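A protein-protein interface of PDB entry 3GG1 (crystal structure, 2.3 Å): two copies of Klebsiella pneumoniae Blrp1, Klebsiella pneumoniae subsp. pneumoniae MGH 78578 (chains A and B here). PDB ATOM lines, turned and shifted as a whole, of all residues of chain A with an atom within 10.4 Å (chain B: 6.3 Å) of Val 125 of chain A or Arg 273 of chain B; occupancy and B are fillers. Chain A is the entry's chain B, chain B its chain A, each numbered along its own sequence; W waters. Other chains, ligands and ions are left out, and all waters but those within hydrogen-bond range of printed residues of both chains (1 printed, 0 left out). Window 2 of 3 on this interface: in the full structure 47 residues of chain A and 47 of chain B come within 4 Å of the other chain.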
ATOM      1  N   ALA A  91     -18.094   3.339  16.989  1.00  0.00           N
ATOM      2  CA  ALA A  91     -17.500   2.241  16.222  1.00  0.00           C
ATOM      3  C   ALA A  91     -18.400   1.765  15.083  1.00  0.00           C
ATOM      4  O   ALA A  91     -17.919   1.174  14.121  1.00  0.00           O
ATOM      5  CB  ALA A  91     -17.178   1.082  17.144  1.00  0.00           C
ATOM      6  N   TYR A  92     -19.703   2.007  15.208  1.00  0.00           N
ATOM      7  CA  TYR A  92     -20.672   1.604  14.194  1.00  0.00           C
ATOM      8  C   TYR A  92     -21.961   2.407  14.343  1.00  0.00           C
ATOM      9  O   TYR A  92     -22.236   2.959  15.406  1.00  0.00           O
ATOM     10  CB  TYR A  92     -20.972   0.107  14.315  1.00  0.00           C
ATOM     11  CG  TYR A  92     -21.647  -0.281  15.617  1.00  0.00           C
ATOM     12  CD1 TYR A  92     -20.909  -0.431  16.791  1.00  0.00           C
ATOM     13  CD2 TYR A  92     -23.022  -0.491  15.676  1.00  0.00           C
ATOM     14  CE1 TYR A  92     -21.526  -0.781  17.988  1.00  0.00           C
ATOM     15  CE2 TYR A  92     -23.645  -0.842  16.864  1.00  0.00           C
ATOM     16  CZ  TYR A  92     -22.894  -0.987  18.014  1.00  0.00           C
ATOM     17  OH  TYR A  92     -23.512  -1.332  19.191  1.00  0.00           O
ATOM     18  N   ARG A  94     -25.662   2.633  15.069  1.00  0.00           N
ATOM     19  CA  ARG A  94     -26.779   1.920  15.691  1.00  0.00           C
ATOM     20  C   ARG A  94     -28.003   2.002  14.778  1.00  0.00           C
ATOM     21  O   ARG A  94     -28.656   0.994  14.513  1.00  0.00           O
ATOM     22  CB  ARG A  94     -27.115   2.511  17.067  1.00  0.00           C
ATOM     23  CG  ARG A  94     -26.255   1.995  18.219  1.00  0.00           C
ATOM     24  CD  ARG A  94     -24.790   2.370  18.071  1.00  0.00           C
ATOM     25  NE  ARG A  94     -24.023   2.100  19.285  1.00  0.00           N
ATOM     26  CZ  ARG A  94     -22.709   2.291  19.412  1.00  0.00           C
ATOM     27  NH1 ARG A  94     -21.992   2.754  18.396  1.00  0.00           N
ATOM     28  NH2 ARG A  94     -22.102   2.019  20.563  1.00  0.00           N
ATOM     29  N   SER A 121     -32.701  -0.703  14.636  1.00  0.00           N
ATOM     30  CA  SER A 121     -31.388  -0.526  15.240  1.00  0.00           C
ATOM     31  C   SER A 121     -30.779  -1.819  15.760  1.00  0.00           C
ATOM     32  O   SER A 121     -31.490  -2.753  16.134  1.00  0.00           O
ATOM     33  CB  SER A 121     -31.459   0.492  16.376  1.00  0.00           C
ATOM     34  OG  SER A 121     -32.292   0.021  17.419  1.00  0.00           O
ATOM     35  N   THR A 122     -29.448  -1.841  15.776  1.00  0.00           N
ATOM     36  CA  THR A 122     -28.655  -2.971  16.249  1.00  0.00           C
ATOM     37  C   THR A 122     -27.658  -2.433  17.269  1.00  0.00           C
ATOM     38  O   THR A 122     -27.166  -1.314  17.113  1.00  0.00           O
ATOM     39  CB  THR A 122     -27.875  -3.619  15.092  1.00  0.00           C
ATOM     40  OG1 THR A 122     -27.022  -2.638  14.483  1.00  0.00           O
ATOM     41  CG2 THR A 122     -28.828  -4.181  14.033  1.00  0.00           C
ATOM     42  N   PHE A 123     -27.360  -3.219  18.304  1.00  0.00           N
ATOM     43  CA  PHE A 123     -26.482  -2.770  19.389  1.00  0.00           C
ATOM     44  C   PHE A 123     -25.376  -3.779  19.709  1.00  0.00           C
ATOM     45  O   PHE A 123     -25.068  -4.033  20.875  1.00  0.00           O
ATOM     46  CB  PHE A 123     -27.313  -2.460  20.644  1.00  0.00           C
ATOM     47  CG  PHE A 123     -28.245  -1.293  20.475  1.00  0.00           C
ATOM     48  CD1 PHE A 123     -27.792   0.004  20.667  1.00  0.00           C
ATOM     49  CD2 PHE A 123     -29.569  -1.490  20.117  1.00  0.00           C
ATOM     50  CE1 PHE A 123     -28.645   1.088  20.508  1.00  0.00           C
ATOM     51  CE2 PHE A 123     -30.429  -0.413  19.957  1.00  0.00           C
ATOM     52  CZ  PHE A 123     -29.967   0.878  20.151  1.00  0.00           C
ATOM     53  N   GLY A 124     -24.768  -4.338  18.666  1.00  0.00           N
ATOM     54  CA  GLY A 124     -23.687  -5.307  18.832  1.00  0.00           C
ATOM     55  C   GLY A 124     -24.182  -6.677  19.258  1.00  0.00           C
ATOM     56  O   GLY A 124     -25.383  -6.946  19.233  1.00  0.00           O
ATOM     57  N   VAL A 125     -23.249  -7.540  19.654  1.00  0.00           N
ATOM     58  CA  VAL A 125     -23.569  -8.927  20.007  1.00  0.00           C
ATOM     59  C   VAL A 125     -24.232  -9.072  21.378  1.00  0.00           C
ATOM     60  O   VAL A 125     -24.974 -10.029  21.605  1.00  0.00           O
ATOM     61  CB  VAL A 125     -22.319  -9.857  19.941  1.00  0.00           C
ATOM     62  CG1 VAL A 125     -21.837  -9.991  18.508  1.00  0.00           C
ATOM     63  CG2 VAL A 125     -21.187  -9.361  20.851  1.00  0.00           C
ATOM     64  N   THR A 126     -23.968  -8.130  22.283  1.00  0.00           N
ATOM     65  CA  THR A 126     -24.508  -8.188  23.643  1.00  0.00           C
ATOM     66  C   THR A 126     -25.879  -7.510  23.739  1.00  0.00           C
ATOM     67  O   THR A 126     -26.344  -6.877  22.789  1.00  0.00           O
ATOM     68  CB  THR A 126     -23.538  -7.552  24.673  1.00  0.00           C
ATOM     69  OG1 THR A 126     -23.486  -6.127  24.493  1.00  0.00           O
ATOM     70  CG2 THR A 126     -22.136  -8.140  24.530  1.00  0.00           C
ATOM     71  N   GLU A 127     -26.507  -7.650  24.904  1.00  0.00           N
ATOM     72  CA  GLU A 127     -27.843  -7.113  25.166  1.00  0.00           C
ATOM     73  C   GLU A 127     -27.863  -5.583  24.983  1.00  0.00           C
ATOM     74  O   GLU A 127     -26.947  -4.901  25.439  1.00  0.00           O
ATOM     75  CB  GLU A 127     -28.272  -7.479  26.597  1.00  0.00           C
ATOM     76  CG  GLU A 127     -29.766  -7.713  26.781  1.00  0.00           C
ATOM     77  CD  GLU A 127     -30.241  -9.037  26.199  1.00  0.00           C
ATOM     78  OE1 GLU A 127     -29.637 -10.083  26.521  1.00  0.00           O
ATOM     79  OE2 GLU A 127     -31.228  -9.030  25.429  1.00  0.00           O
ATOM     80  N   PRO A 128     -28.901  -5.042  24.310  1.00  0.00           N
ATOM     81  CA  PRO A 128     -29.014  -3.599  24.057  1.00  0.00           C
ATOM     82  C   PRO A 128     -28.802  -2.720  25.292  1.00  0.00           C
ATOM     83  O   PRO A 128     -28.209  -1.642  25.191  1.00  0.00           O
ATOM     84  CB  PRO A 128     -30.450  -3.446  23.551  1.00  0.00           C
ATOM     85  CG  PRO A 128     -30.773  -4.744  22.940  1.00  0.00           C
ATOM     86  CD  PRO A 128     -30.033  -5.784  23.722  1.00  0.00           C
ATOM     87  N   VAL A 129     -29.278  -3.191  26.444  1.00  0.00           N
ATOM     88  CA  VAL A 129     -29.130  -2.474  27.710  1.00  0.00           C
ATOM     89  C   VAL A 129     -27.659  -2.203  28.071  1.00  0.00           C
ATOM     90  O   VAL A 129     -27.378  -1.311  28.865  1.00  0.00           O
ATOM     91  CB  VAL A 129     -29.853  -3.223  28.869  1.00  0.00           C
ATOM     92  CG1 VAL A 129     -29.098  -4.496  29.264  1.00  0.00           C
ATOM     93  CG2 VAL A 129     -30.055  -2.305  30.067  1.00  0.00           C
ATOM     94  N   ASN A 130     -26.732  -2.963  27.481  1.00  0.00           N
ATOM     95  CA  ASN A 130     -25.292  -2.699  27.625  1.00  0.00           C
ATOM     96  C   ASN A 130     -24.782  -1.504  26.813  1.00  0.00           C
ATOM     97  O   ASN A 130     -23.600  -1.171  26.897  1.00  0.00           O
ATOM     98  CB  ASN A 130     -24.475  -3.936  27.235  1.00  0.00           C
ATOM     99  CG  ASN A 130     -24.678  -5.097  28.187  1.00  0.00           C
ATOM    100  OD1 ASN A 130     -24.665  -4.925  29.408  1.00  0.00           O
ATOM    101  ND2 ASN A 130     -24.848  -6.291  27.635  1.00  0.00           N
ATOM    102  N   ASP A 131     -25.658  -0.861  26.039  1.00  0.00           N
ATOM    103  CA  ASP A 131     -25.278   0.289  25.227  1.00  0.00           C
ATOM    104  C   ASP A 131     -25.803   1.605  25.808  1.00  0.00           C
ATOM    105  O   ASP A 131     -26.994   1.735  26.086  1.00  0.00           O
ATOM    106  CB  ASP A 131     -25.801   0.121  23.805  1.00  0.00           C
ATOM    107  CG  ASP A 131     -25.085   1.008  22.828  1.00  0.00           C
ATOM    108  OD1 ASP A 131     -25.657   2.036  22.417  1.00  0.00           O
ATOM    109  OD2 ASP A 131     -23.932   0.682  22.488  1.00  0.00           O
ATOM    110  N   GLY B 240     -20.182 -16.347  24.184  1.00  0.00           N
ATOM    111  CA  GLY B 240     -21.504 -16.127  23.606  1.00  0.00           C
ATOM    112  C   GLY B 240     -21.838 -14.653  23.475  1.00  0.00           C
ATOM    113  O   GLY B 240     -21.106 -13.904  22.833  1.00  0.00           O
ATOM    114  N   LYS B 241     -22.944 -14.240  24.088  1.00  0.00           N
ATOM    115  CA  LYS B 241     -23.395 -12.851  24.037  1.00  0.00           C
ATOM    116  C   LYS B 241     -23.087 -12.094  25.335  1.00  0.00           C
ATOM    117  O   LYS B 241     -23.624 -11.008  25.563  1.00  0.00           O
ATOM    118  CB  LYS B 241     -24.901 -12.800  23.751  1.00  0.00           C
ATOM    119  CG  LYS B 241     -25.343 -13.631  22.551  1.00  0.00           C
ATOM    120  CD  LYS B 241     -26.791 -13.346  22.190  1.00  0.00           C
ATOM    121  CE  LYS B 241     -27.241 -14.141  20.969  1.00  0.00           C
ATOM    122  NZ  LYS B 241     -27.765 -15.487  21.332  1.00  0.00           N
ATOM    123  N   HIS B 242     -22.225 -12.661  26.177  1.00  0.00           N
ATOM    124  CA  HIS B 242     -21.862 -12.039  27.447  1.00  0.00           C
ATOM    125  C   HIS B 242     -20.701 -11.064  27.280  1.00  0.00           C
ATOM    126  O   HIS B 242     -19.868 -11.219  26.388  1.00  0.00           O
ATOM    127  CB  HIS B 242     -21.484 -13.104  28.481  1.00  0.00           C
ATOM    128  CG  HIS B 242     -22.614 -14.010  28.855  1.00  0.00           C
ATOM    129  ND1 HIS B 242     -22.728 -15.296  28.376  1.00  0.00           N
ATOM    130  CD2 HIS B 242     -23.682 -13.814  29.664  1.00  0.00           C
ATOM    131  CE1 HIS B 242     -23.818 -15.854  28.874  1.00  0.00           C
ATOM    132  NE2 HIS B 242     -24.416 -14.975  29.657  1.00  0.00           N
ATOM    133  N   MET B 264      -7.325  -5.389  20.189  1.00  0.00           N
ATOM    134  CA  MET B 264      -8.272  -5.687  19.108  1.00  0.00           C
ATOM    135  C   MET B 264      -7.900  -6.975  18.365  1.00  0.00           C
ATOM    136  O   MET B 264      -8.733  -7.861  18.192  1.00  0.00           O
ATOM    137  CB  MET B 264      -8.313  -4.517  18.114  1.00  0.00           C
ATOM    138  CG  MET B 264      -9.638  -4.331  17.372  1.00  0.00           C
ATOM    139  SD  MET B 264     -11.088  -3.978  18.407  1.00  0.00           S
ATOM    140  CE  MET B 264     -10.352  -3.107  19.757  1.00  0.00           C
ATOM    141  N   LEU B 267      -8.289 -10.091  20.807  1.00  0.00           N
ATOM    142  CA  LEU B 267      -9.672 -10.458  21.123  1.00  0.00           C
ATOM    143  C   LEU B 267     -10.387 -11.029  19.899  1.00  0.00           C
ATOM    144  O   LEU B 267     -11.181 -11.962  20.030  1.00  0.00           O
ATOM    145  CB  LEU B 267     -10.444  -9.269  21.727  1.00  0.00           C
ATOM    146  CG  LEU B 267     -10.903  -8.105  20.839  1.00  0.00           C
ATOM    147  CD1 LEU B 267     -12.267  -8.372  20.197  1.00  0.00           C
ATOM    148  CD2 LEU B 267     -10.958  -6.814  21.645  1.00  0.00           C
ATOM    149  N   LEU B 268     -10.097 -10.479  18.721  1.00  0.00           N
ATOM    150  CA  LEU B 268     -10.668 -10.978  17.466  1.00  0.00           C
ATOM    151  C   LEU B 268     -10.195 -12.397  17.164  1.00  0.00           C
ATOM    152  O   LEU B 268     -10.992 -13.248  16.762  1.00  0.00           O
ATOM    153  CB  LEU B 268     -10.320 -10.049  16.294  1.00  0.00           C
ATOM    154  CG  LEU B 268     -11.054  -8.704  16.275  1.00  0.00           C
ATOM    155  CD1 LEU B 268     -10.346  -7.696  15.374  1.00  0.00           C
ATOM    156  CD2 LEU B 268     -12.502  -8.886  15.843  1.00  0.00           C
ATOM    157  N   GLY B 271     -11.985 -15.026  18.824  1.00  0.00           N
ATOM    158  CA  GLY B 271     -13.376 -15.135  18.396  1.00  0.00           C
ATOM    159  C   GLY B 271     -14.325 -14.233  19.163  1.00  0.00           C
ATOM    160  O   GLY B 271     -15.491 -14.579  19.343  1.00  0.00           O
ATOM    161  N   LEU B 272     -13.832 -13.079  19.606  1.00  0.00           N
ATOM    162  CA  LEU B 272     -14.646 -12.121  20.354  1.00  0.00           C
ATOM    163  C   LEU B 272     -14.898 -10.871  19.524  1.00  0.00           C
ATOM    164  O   LEU B 272     -14.229 -10.637  18.519  1.00  0.00           O
ATOM    165  CB  LEU B 272     -13.958 -11.735  21.668  1.00  0.00           C
ATOM    166  CG  LEU B 272     -13.598 -12.883  22.615  1.00  0.00           C
ATOM    167  CD1 LEU B 272     -12.723 -12.391  23.751  1.00  0.00           C
ATOM    168  CD2 LEU B 272     -14.852 -13.544  23.161  1.00  0.00           C
ATOM    169  N   ARG B 273     -15.871 -10.076  19.953  1.00  0.00           N
ATOM    170  CA  ARG B 273     -16.176  -8.799  19.315  1.00  0.00           C
ATOM    171  C   ARG B 273     -15.719  -7.644  20.208  1.00  0.00           C
ATOM    172  O   ARG B 273     -15.753  -7.765  21.430  1.00  0.00           O
ATOM    173  CB  ARG B 273     -17.677  -8.691  19.029  1.00  0.00           C
ATOM    174  CG  ARG B 273     -18.188  -9.641  17.945  1.00  0.00           C
ATOM    175  CD  ARG B 273     -17.515  -9.397  16.594  1.00  0.00           C
ATOM    176  NE  ARG B 273     -17.585  -7.989  16.203  1.00  0.00           N
ATOM    177  CZ  ARG B 273     -16.817  -7.410  15.281  1.00  0.00           C
ATOM    178  NH1 ARG B 273     -15.888  -8.102  14.623  1.00  0.00           N
ATOM    179  NH2 ARG B 273     -16.978  -6.114  15.019  1.00  0.00           N
ATOM    180  N   PRO B 274     -15.282  -6.523  19.597  1.00  0.00           N
ATOM    181  CA  PRO B 274     -14.852  -5.332  20.341  1.00  0.00           C
ATOM    182  C   PRO B 274     -15.881  -4.859  21.366  1.00  0.00           C
ATOM    183  O   PRO B 274     -15.543  -4.683  22.533  1.00  0.00           O
ATOM    184  CB  PRO B 274     -14.674  -4.273  19.245  1.00  0.00           C
ATOM    185  CG  PRO B 274     -14.459  -5.029  18.002  1.00  0.00           C
ATOM    186  CD  PRO B 274     -15.168  -6.331  18.140  1.00  0.00           C
ATOM    187  N   ASP B 275     -17.127  -4.685  20.924  1.00  0.00           N
ATOM    188  CA  ASP B 275     -18.233  -4.223  21.786  1.00  0.00           C
ATOM    189  C   ASP B 275     -18.547  -5.154  22.961  1.00  0.00           C
ATOM    190  O   ASP B 275     -19.296  -4.790  23.866  1.00  0.00           O
ATOM    191  CB  ASP B 275     -19.509  -3.999  20.957  1.00  0.00           C
ATOM    192  CG  ASP B 275     -19.951  -5.246  20.210  1.00  0.00           C
ATOM    193  OD1 ASP B 275     -19.316  -5.583  19.186  1.00  0.00           O
ATOM    194  OD2 ASP B 275     -20.930  -5.885  20.646  1.00  0.00           O
ATOM    195  N   GLN B 276     -17.970  -6.351  22.930  1.00  0.00           N
ATOM    196  CA  GLN B 276     -18.166  -7.360  23.951  1.00  0.00           C
ATOM    197  C   GLN B 276     -17.103  -7.275  25.053  1.00  0.00           C
ATOM    198  O   GLN B 276     -17.237  -7.913  26.098  1.00  0.00           O
ATOM    199  CB  GLN B 276     -18.098  -8.725  23.274  1.00  0.00           C
ATOM    200  CG  GLN B 276     -18.762  -9.838  24.011  1.00  0.00           C
ATOM    201  CD  GLN B 276     -18.722 -11.138  23.239  1.00  0.00           C
ATOM    202  OE1 GLN B 276     -18.004 -11.269  22.249  1.00  0.00           O
ATOM    203  NE2 GLN B 276     -19.490 -12.113  23.699  1.00  0.00           N
ATOM    204  N   VAL B 277     -16.049  -6.494  24.812  1.00  0.00           N
ATOM    205  CA  VAL B 277     -14.922  -6.392  25.738  1.00  0.00           C
ATOM    206  C   VAL B 277     -14.900  -5.025  26.424  1.00  0.00           C
ATOM    207  O   VAL B 277     -14.942  -3.982  25.767  1.00  0.00           O
ATOM    208  CB  VAL B 277     -13.582  -6.626  25.019  1.00  0.00           C
ATOM    209  CG1 VAL B 277     -12.414  -6.546  26.003  1.00  0.00           C
ATOM    210  CG2 VAL B 277     -13.596  -7.976  24.304  1.00  0.00           C
ATOM    211  N   MET B 305     -14.580  -0.938  21.853  1.00  0.00           N
ATOM    212  CA  MET B 305     -14.484  -1.513  23.190  1.00  0.00           C
ATOM    213  C   MET B 305     -15.081  -0.546  24.200  1.00  0.00           C
ATOM    214  O   MET B 305     -15.194   0.651  23.934  1.00  0.00           O
ATOM    215  CB  MET B 305     -13.034  -1.831  23.549  1.00  0.00           C
ATOM    216  CG  MET B 305     -12.440  -2.942  22.710  1.00  0.00           C
ATOM    217  SD  MET B 305     -10.787  -3.435  23.234  1.00  0.00           S
ATOM    218  CE  MET B 305      -9.804  -2.042  22.713  1.00  0.00           C
HETATM  219  O   HOH W   1     -21.046  -4.765  25.562  1.00  0.00           O
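The side-chain carboxylate of Asp 275 of chain B lies within hydrogen-bond range of the backbone NH of Val 125 of chain A (3.0 Å).
O of Gly 240 of chain B is in hydrogen-bond range of NE2 of Gln 276 of chain B, 2.6 Å away.
O of His 242 of chain B lies within hydrogen-bond range of NE2 of Gln 276 of chain B, 2.9 Å away.
N of Arg 273 of chain B is in hydrogen-bond range of OE1 of Gln 276 of chain B (3.4 Å).
OH of Tyr 92 of chain A sits at hydrogen-bond distance from N of Gly 124 of chain A, at 3.3 Å.
The side-chain hydroxyl of Thr 126 of chain A sits at hydrogen-bond distance from the side-chain amide nitrogen of Asn 130 of chain A, at 3.4 Å.
OD2 of Asp 275 of chain B touches CA of Gly 124 of chain A, at 3.4 Å.
Lys 241 of chain B touches Val 125 of chain A.
Arg 273 of chain B touches Val 125 of chain A.
Val 125 of chain A touches Gln 276 of chain B (CG2 to CD, 3.9 Å).
Lys 241 of chain B touches Thr 126 of chain A.
Thr 126 of chain A touches Gln 276 of chain B.
No residue of chain A comes within 4 Å of Pro 274 of chain B.
Asp 275 of chain B touches just these residues of chain A: Gly 124 and Val 125.
No residue of chain A comes within 4 Å of Val 277 of chain B.
Printed residues of chain B within 4 Å of Thr 126 of chain A: Lys 241 and Gln 276.
Of the printed residues of chain B, Gly 124 of chain A touches Asp 275.
Met 264 of chain B touches none of the printed residues of chain A.
The nearest residue of chain B that does not touch Val 125 of chain A is Gly 240 of chain B (5.0 Å).
The nearest printed residue of chain B that does not touch Thr 126 of chain A is Asp 275 of chain B (4.1 Å).
Along chain B the printed residues that touch a printed residue of chain A span positions 241 to 276.
Printed residues of chain A that touch a printed residue of chain B: Gly 124, Val 125 and Thr 126.
Hydrophobic or aromatic side chains of chain A within 4 Å of the printed part of chain B: Val 125.
Along chain A the printed residues that touch a printed residue of chain B span positions 124 to 126.
No position is printed for both chains.
Water W1 lies within hydrogen-bond range of O of Asp 275 of chain B and OG1 of Thr 126 of chain A.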
